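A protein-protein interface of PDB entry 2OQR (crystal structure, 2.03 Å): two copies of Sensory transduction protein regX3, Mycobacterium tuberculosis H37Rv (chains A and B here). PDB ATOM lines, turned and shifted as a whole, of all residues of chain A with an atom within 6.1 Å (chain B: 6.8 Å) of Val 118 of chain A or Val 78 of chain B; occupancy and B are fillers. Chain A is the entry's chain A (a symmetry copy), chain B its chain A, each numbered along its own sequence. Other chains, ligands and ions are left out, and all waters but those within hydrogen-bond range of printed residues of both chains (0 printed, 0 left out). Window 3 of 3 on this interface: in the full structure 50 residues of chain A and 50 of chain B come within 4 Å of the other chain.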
ATOM      1  N   ASP A  99      14.305  18.870  14.296  1.00  0.00           N
ATOM      2  CA  ASP A  99      14.357  18.274  12.965  1.00  0.00           C
ATOM      3  C   ASP A  99      15.743  18.417  12.343  1.00  0.00           C
ATOM      4  O   ASP A  99      16.080  17.719  11.403  1.00  0.00           O
ATOM      5  CB  ASP A  99      13.322  18.912  12.041  1.00  0.00           C
ATOM      6  CG  ASP A  99      11.914  18.506  12.386  1.00  0.00           C
ATOM      7  OD1 ASP A  99      11.478  17.479  11.839  1.00  0.00           O
ATOM      8  OD2 ASP A  99      11.267  19.193  13.214  1.00  0.00           O
ATOM      9  N   ALA A 113      15.691  28.461   1.467  1.00  0.00           N
ATOM     10  CA  ALA A 113      15.590  27.377   0.447  1.00  0.00           C
ATOM     11  C   ALA A 113      15.285  26.040   1.093  1.00  0.00           C
ATOM     12  O   ALA A 113      14.525  25.209   0.547  1.00  0.00           O
ATOM     13  CB  ALA A 113      16.896  27.304  -0.388  1.00  0.00           C
ATOM     14  N   ARG A 114      15.835  25.796   2.268  1.00  0.00           N
ATOM     15  CA  ARG A 114      15.546  24.547   2.982  1.00  0.00           C
ATOM     16  C   ARG A 114      14.132  24.516   3.585  1.00  0.00           C
ATOM     17  O   ARG A 114      13.460  23.500   3.597  1.00  0.00           O
ATOM     18  CB  ARG A 114      16.569  24.342   4.071  1.00  0.00           C
ATOM     19  CG  ARG A 114      17.960  24.199   3.487  1.00  0.00           C
ATOM     20  CD  ARG A 114      18.930  23.942   4.550  1.00  0.00           C
ATOM     21  NE  ARG A 114      18.599  22.697   5.214  1.00  0.00           N
ATOM     22  CZ  ARG A 114      19.251  22.217   6.256  1.00  0.00           C
ATOM     23  NH1 ARG A 114      20.278  22.884   6.773  1.00  0.00           N
ATOM     24  NH2 ARG A 114      18.854  21.075   6.788  1.00  0.00           N
ATOM     25  N   ILE A 115      13.672  25.662   4.071  1.00  0.00           N
ATOM     26  CA  ILE A 115      12.279  25.764   4.500  1.00  0.00           C
ATOM     27  C   ILE A 115      11.334  25.464   3.351  1.00  0.00           C
ATOM     28  O   ILE A 115      10.410  24.687   3.517  1.00  0.00           O
ATOM     29  CB  ILE A 115      11.987  27.153   5.172  1.00  0.00           C
ATOM     30  CG1 ILE A 115      12.763  27.268   6.476  1.00  0.00           C
ATOM     31  CG2 ILE A 115      10.506  27.296   5.440  1.00  0.00           C
ATOM     32  CD1 ILE A 115      12.741  28.658   7.139  1.00  0.00           C
ATOM     33  N   ARG A 116      11.540  26.073   2.177  1.00  0.00           N
ATOM     34  CA  ARG A 116      10.648  25.807   1.023  1.00  0.00           C
ATOM     35  C   ARG A 116      10.636  24.346   0.642  1.00  0.00           C
ATOM     36  O   ARG A 116       9.597  23.768   0.307  1.00  0.00           O
ATOM     37  CB  ARG A 116      11.042  26.632  -0.232  1.00  0.00           C
ATOM     38  CG  ARG A 116      11.079  28.122  -0.072  1.00  0.00           C
ATOM     39  CD  ARG A 116      11.683  28.722  -1.329  1.00  0.00           C
ATOM     40  NE  ARG A 116      11.881  30.156  -1.272  1.00  0.00           N
ATOM     41  CZ  ARG A 116      10.981  31.091  -1.562  1.00  0.00           C
ATOM     42  NH1 ARG A 116       9.752  30.813  -1.917  1.00  0.00           N
ATOM     43  NH2 ARG A 116      11.318  32.329  -1.496  1.00  0.00           N
ATOM     44  N   ALA A 117      11.802  23.715   0.734  1.00  0.00           N
ATOM     45  CA  ALA A 117      11.971  22.310   0.416  1.00  0.00           C
ATOM     46  C   ALA A 117      11.170  21.399   1.368  1.00  0.00           C
ATOM     47  O   ALA A 117      10.485  20.454   0.957  1.00  0.00           O
ATOM     48  CB  ALA A 117      13.471  21.949   0.495  1.00  0.00           C
ATOM     49  N   VAL A 118      11.272  21.674   2.658  1.00  0.00           N
ATOM     50  CA  VAL A 118      10.495  20.935   3.658  1.00  0.00           C
ATOM     51  C   VAL A 118       9.001  21.021   3.342  1.00  0.00           C
ATOM     52  O   VAL A 118       8.277  20.034   3.388  1.00  0.00           O
ATOM     53  CB  VAL A 118      10.722  21.529   5.083  1.00  0.00           C
ATOM     54  CG1 VAL A 118       9.862  20.818   6.091  1.00  0.00           C
ATOM     55  CG2 VAL A 118      12.154  21.376   5.482  1.00  0.00           C
ATOM     56  N   LEU A 119       8.547  22.227   3.035  1.00  0.00           N
ATOM     57  CA  LEU A 119       7.148  22.458   2.770  1.00  0.00           C
ATOM     58  C   LEU A 119       6.648  21.759   1.515  1.00  0.00           C
ATOM     59  O   LEU A 119       5.460  21.549   1.404  1.00  0.00           O
ATOM     60  CB  LEU A 119       6.848  23.946   2.714  1.00  0.00           C
ATOM     61  CG  LEU A 119       7.090  24.684   4.031  1.00  0.00           C
ATOM     62  CD1 LEU A 119       6.912  26.151   3.803  1.00  0.00           C
ATOM     63  CD2 LEU A 119       6.186  24.190   5.162  1.00  0.00           C
ATOM     64  N   ARG A 120       7.534  21.412   0.577  1.00  0.00           N
ATOM     65  CA  ARG A 120       7.161  20.605  -0.597  1.00  0.00           C
ATOM     66  C   ARG A 120       7.637  19.166  -0.499  1.00  0.00           C
ATOM     67  O   ARG A 120       7.708  18.479  -1.519  1.00  0.00           O
ATOM     68  CB  ARG A 120       7.707  21.219  -1.892  1.00  0.00           C
ATOM     69  CG  ARG A 120       9.228  21.175  -2.078  1.00  0.00           C
ATOM     70  CD  ARG A 120       9.667  21.851  -3.372  1.00  0.00           C
ATOM     71  NE  ARG A 120      10.960  22.531  -3.226  1.00  0.00           N
ATOM     72  CZ  ARG A 120      12.124  21.906  -3.237  1.00  0.00           C
ATOM     73  NH1 ARG A 120      12.180  20.582  -3.332  1.00  0.00           N
ATOM     74  NH2 ARG A 120      13.247  22.587  -3.111  1.00  0.00           N
ATOM     75  N   ARG A 121       7.990  18.731   0.703  1.00  0.00           N
ATOM     76  CA  ARG A 121       8.492  17.377   0.945  1.00  0.00           C
ATOM     77  C   ARG A 121       9.606  17.056  -0.041  1.00  0.00           C
ATOM     78  O   ARG A 121       9.546  16.087  -0.809  1.00  0.00           O
ATOM     79  CB  ARG A 121       7.350  16.368   0.893  1.00  0.00           C
ATOM     80  CG  ARG A 121       6.338  16.540   2.031  1.00  0.00           C
ATOM     81  CD  ARG A 121       5.110  17.397   1.648  1.00  0.00           C
ATOM     82  NE  ARG A 121       3.916  16.572   1.378  1.00  0.00           N
ATOM     83  CZ  ARG A 121       2.687  17.043   1.130  1.00  0.00           C
ATOM     84  NH1 ARG A 121       1.685  16.189   0.910  1.00  0.00           N
ATOM     85  NH2 ARG A 121       2.447  18.357   1.101  1.00  0.00           N
ATOM     86  N   GLY A 122      10.601  17.939  -0.060  1.00  0.00           N
ATOM     87  CA  GLY A 122      11.742  17.787  -0.945  1.00  0.00           C
ATOM     88  C   GLY A 122      12.456  16.447  -0.799  1.00  0.00           C
ATOM     89  O   GLY A 122      12.561  15.912   0.295  1.00  0.00           O
ATOM     90  N   ALA B  49       3.285  28.113  15.389  1.00  0.00           N
ATOM     91  CA  ALA B  49       4.288  28.350  14.348  1.00  0.00           C
ATOM     92  C   ALA B  49       4.419  27.109  13.548  1.00  0.00           C
ATOM     93  O   ALA B  49       4.283  26.001  14.076  1.00  0.00           O
ATOM     94  CB  ALA B  49       5.643  28.712  14.923  1.00  0.00           C
ATOM     95  N   ASP B  50       4.651  27.289  12.259  1.00  0.00           N
ATOM     96  CA  ASP B  50       4.910  26.146  11.381  1.00  0.00           C
ATOM     97  C   ASP B  50       6.370  25.719  11.391  1.00  0.00           C
ATOM     98  O   ASP B  50       6.682  24.548  11.259  1.00  0.00           O
ATOM     99  CB  ASP B  50       4.486  26.534   9.992  1.00  0.00           C
ATOM    100  CG  ASP B  50       3.009  26.896   9.946  1.00  0.00           C
ATOM    101  OD1 ASP B  50       2.196  25.980  10.201  1.00  0.00           O
ATOM    102  OD2 ASP B  50       2.685  28.073   9.694  1.00  0.00           O
ATOM    103  N   ILE B  51       7.251  26.702  11.527  1.00  0.00           N
ATOM    104  CA  ILE B  51       8.696  26.484  11.542  1.00  0.00           C
ATOM    105  C   ILE B  51       9.212  27.199  12.741  1.00  0.00           C
ATOM    106  O   ILE B  51       8.828  28.344  12.968  1.00  0.00           O
ATOM    107  CB  ILE B  51       9.421  27.118  10.298  1.00  0.00           C
ATOM    108  CG1 ILE B  51       8.767  26.692   8.988  1.00  0.00           C
ATOM    109  CG2 ILE B  51      10.946  26.759  10.320  1.00  0.00           C
ATOM    110  CD1 ILE B  51       8.813  25.221   8.737  1.00  0.00           C
ATOM    111  N   VAL B  52      10.090  26.553  13.500  1.00  0.00           N
ATOM    112  CA  VAL B  52      10.778  27.238  14.606  1.00  0.00           C
ATOM    113  C   VAL B  52      12.285  27.152  14.398  1.00  0.00           C
ATOM    114  O   VAL B  52      12.823  26.070  14.205  1.00  0.00           O
ATOM    115  CB  VAL B  52      10.417  26.634  15.991  1.00  0.00           C
ATOM    116  CG1 VAL B  52      11.213  27.351  17.096  1.00  0.00           C
ATOM    117  CG2 VAL B  52       8.920  26.679  16.219  1.00  0.00           C
ATOM    118  N   LEU B  53      12.946  28.306  14.397  1.00  0.00           N
ATOM    119  CA  LEU B  53      14.411  28.399  14.292  1.00  0.00           C
ATOM    120  C   LEU B  53      14.913  28.804  15.668  1.00  0.00           C
ATOM    121  O   LEU B  53      14.603  29.886  16.138  1.00  0.00           O
ATOM    122  CB  LEU B  53      14.777  29.437  13.216  1.00  0.00           C
ATOM    123  CG  LEU B  53      14.092  29.194  11.857  1.00  0.00           C
ATOM    124  CD1 LEU B  53      14.431  30.288  10.851  1.00  0.00           C
ATOM    125  CD2 LEU B  53      14.416  27.835  11.264  1.00  0.00           C
ATOM    126  N   ARG B  71       8.339  20.802  21.368  1.00  0.00           N
ATOM    127  CA  ARG B  71       7.992  19.502  20.815  1.00  0.00           C
ATOM    128  C   ARG B  71       6.889  18.798  21.634  1.00  0.00           C
ATOM    129  O   ARG B  71       6.001  18.168  21.055  1.00  0.00           O
ATOM    130  CB  ARG B  71       9.229  18.620  20.671  1.00  0.00           C
ATOM    131  CG  ARG B  71       8.954  17.271  20.010  1.00  0.00           C
ATOM    132  CD  ARG B  71       8.219  17.427  18.673  1.00  0.00           C
ATOM    133  NE  ARG B  71       9.117  17.882  17.620  1.00  0.00           N
ATOM    134  CZ  ARG B  71       8.821  18.724  16.629  1.00  0.00           C
ATOM    135  NH1 ARG B  71       7.617  19.260  16.524  1.00  0.00           N
ATOM    136  NH2 ARG B  71       9.756  19.023  15.723  1.00  0.00           N
ATOM    137  N   SER B  75       3.630  17.922  17.593  1.00  0.00           N
ATOM    138  CA  SER B  75       4.517  17.258  16.653  1.00  0.00           C
ATOM    139  C   SER B  75       4.557  17.920  15.271  1.00  0.00           C
ATOM    140  O   SER B  75       5.314  17.494  14.425  1.00  0.00           O
ATOM    141  CB  SER B  75       4.115  15.792  16.518  1.00  0.00           C
ATOM    142  OG  SER B  75       2.844  15.663  15.922  1.00  0.00           O
ATOM    143  N   VAL B  76       3.758  18.963  15.038  1.00  0.00           N
ATOM    144  CA  VAL B  76       3.673  19.588  13.699  1.00  0.00           C
ATOM    145  C   VAL B  76       4.865  20.470  13.308  1.00  0.00           C
ATOM    146  O   VAL B  76       5.416  20.267  12.252  1.00  0.00           O
ATOM    147  CB  VAL B  76       2.340  20.340  13.499  1.00  0.00           C
ATOM    148  CG1 VAL B  76       2.345  21.122  12.209  1.00  0.00           C
ATOM    149  CG2 VAL B  76       1.178  19.334  13.505  1.00  0.00           C
ATOM    150  N   PRO B  77       5.271  21.444  14.145  1.00  0.00           N
ATOM    151  CA  PRO B  77       6.322  22.380  13.767  1.00  0.00           C
ATOM    152  C   PRO B  77       7.650  21.720  13.394  1.00  0.00           C
ATOM    153  O   PRO B  77       8.035  20.746  14.019  1.00  0.00           O
ATOM    154  CB  PRO B  77       6.554  23.199  15.047  1.00  0.00           C
ATOM    155  CG  PRO B  77       5.396  22.968  15.880  1.00  0.00           C
ATOM    156  CD  PRO B  77       4.803  21.672  15.515  1.00  0.00           C
ATOM    157  N   VAL B  78       8.298  22.227  12.346  1.00  0.00           N
ATOM    158  CA  VAL B  78       9.689  21.923  12.043  1.00  0.00           C
ATOM    159  C   VAL B  78      10.494  22.750  13.027  1.00  0.00           C
ATOM    160  O   VAL B  78      10.305  23.948  13.119  1.00  0.00           O
ATOM    161  CB  VAL B  78      10.086  22.289  10.572  1.00  0.00           C
ATOM    162  CG1 VAL B  78      11.627  22.176  10.364  1.00  0.00           C
ATOM    163  CG2 VAL B  78       9.378  21.359   9.573  1.00  0.00           C
ATOM    164  N   ILE B  79      11.364  22.110  13.801  1.00  0.00           N
ATOM    165  CA  ILE B  79      12.187  22.819  14.757  1.00  0.00           C
ATOM    166  C   ILE B  79      13.644  22.597  14.353  1.00  0.00           C
ATOM    167  O   ILE B  79      14.116  21.470  14.350  1.00  0.00           O
ATOM    168  CB  ILE B  79      11.989  22.320  16.178  1.00  0.00           C
ATOM    169  CG1 ILE B  79      10.547  22.515  16.664  1.00  0.00           C
ATOM    170  CG2 ILE B  79      12.885  23.081  17.115  1.00  0.00           C
ATOM    171  CD1 ILE B  79      10.269  21.847  17.978  1.00  0.00           C
ATOM    172  N   MET B  80      14.325  23.678  13.984  1.00  0.00           N
ATOM    173  CA  MET B  80      15.744  23.652  13.638  1.00  0.00           C
ATOM    174  C   MET B  80      16.522  24.412  14.698  1.00  0.00           C
ATOM    175  O   MET B  80      16.237  25.594  14.956  1.00  0.00           O
ATOM    176  CB  MET B  80      15.964  24.272  12.258  1.00  0.00           C
ATOM    177  CG  MET B  80      15.106  23.607  11.137  1.00  0.00           C
ATOM    178  SD  MET B  80      15.301  24.457   9.536  1.00  0.00           S
ATOM    179  CE  MET B  80      16.817  23.643   9.012  1.00  0.00           C
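Of the 11 printed residues of chain A, 4 touch a printed residue of chain B. Hydrophobic or aromatic side chains of chain A that line the printed part of chain B: Ile 115 and Val 118. Of the 12 printed residues of chain B, 6 touch a printed residue of chain A. Printed residues of chain B that touch a printed residue of chain A: Ile 51, Arg 71, Pro 77, Val 78, Ile 79 and Met 80. Hydrophobic or aromatic side chains of chain B within 4 Å of the printed part of chain A: Ile 51, Val 78 and Met 80. Among the printed residues, 7 pairs touch across the chains.
N of Asp 99 of chain A is in hydrogen-bond range of O of Ile 79 of chain B (2.6 Å). NH2 of Arg 71 of chain B lies within salt-bridge range of OD2 of Asp 99 of chain A, at 2.9 Å.
Val 118 of chain A touches just one residue of chain B: Val 78 (3.6 Å). Val 78 of chain B touches just these residues of chain A: Asp 99 (3.4 Å) and Val 118 (3.6 Å). Of the printed residues of chain B, Arg 114 of chain A touches Met 80 (3.9 Å). Printed residues of chain A within 4 Å of Pro 77 of chain B: Asp 99 (3.7 Å). Printed residues of chain B within 4 Å of Ile 115 of chain A: Ile 51 (3.997 Å). The nearest residue of chain B that does not touch Val 118 of chain A is Ile 51 of chain B (5.2 Å).
No position is printed for both chains. Of the 7 pairs that touch across the chains among the printed residues, none has its exchanged pair printed and touching as well.
OD2 of Asp 99 of chain A touches O of Pro 77 of chain B, 3.7 Å away. Asp 99 of chain A touches Val 78 of chain B (OD2 to CA, 3.4 Å). CE of Met 80 of chain B touches CZ of Arg 114 of chain A, at 3.9 Å. CG2 of Ile 115 of chain A touches CG1 of Ile 51 of chain B, 3.997 Å away. CG1 of Val 118 of chain A touches CG2 of Val 78 of chain B (3.6 Å).
The backbone NH of Met 80 of chain B is in hydrogen-bond range of the backbone carbonyl oxygen of Val 52 of chain B (2.8 Å). The backbone carbonyl oxygen (O) of Pro 77 of chain B sits at hydrogen-bond distance from the guanidinium group (NH1) of Arg 71 of chain B. The backbone carbonyl oxygen of Val 78 of chain B sits at hydrogen-bond distance from the backbone NH of Val 52 of chain B (2.6 Å). The backbone carbonyl oxygen of Asp 50 of chain B is in hydrogen-bond range of the backbone NH of Val 78 of chain B, at 3.0 Å.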
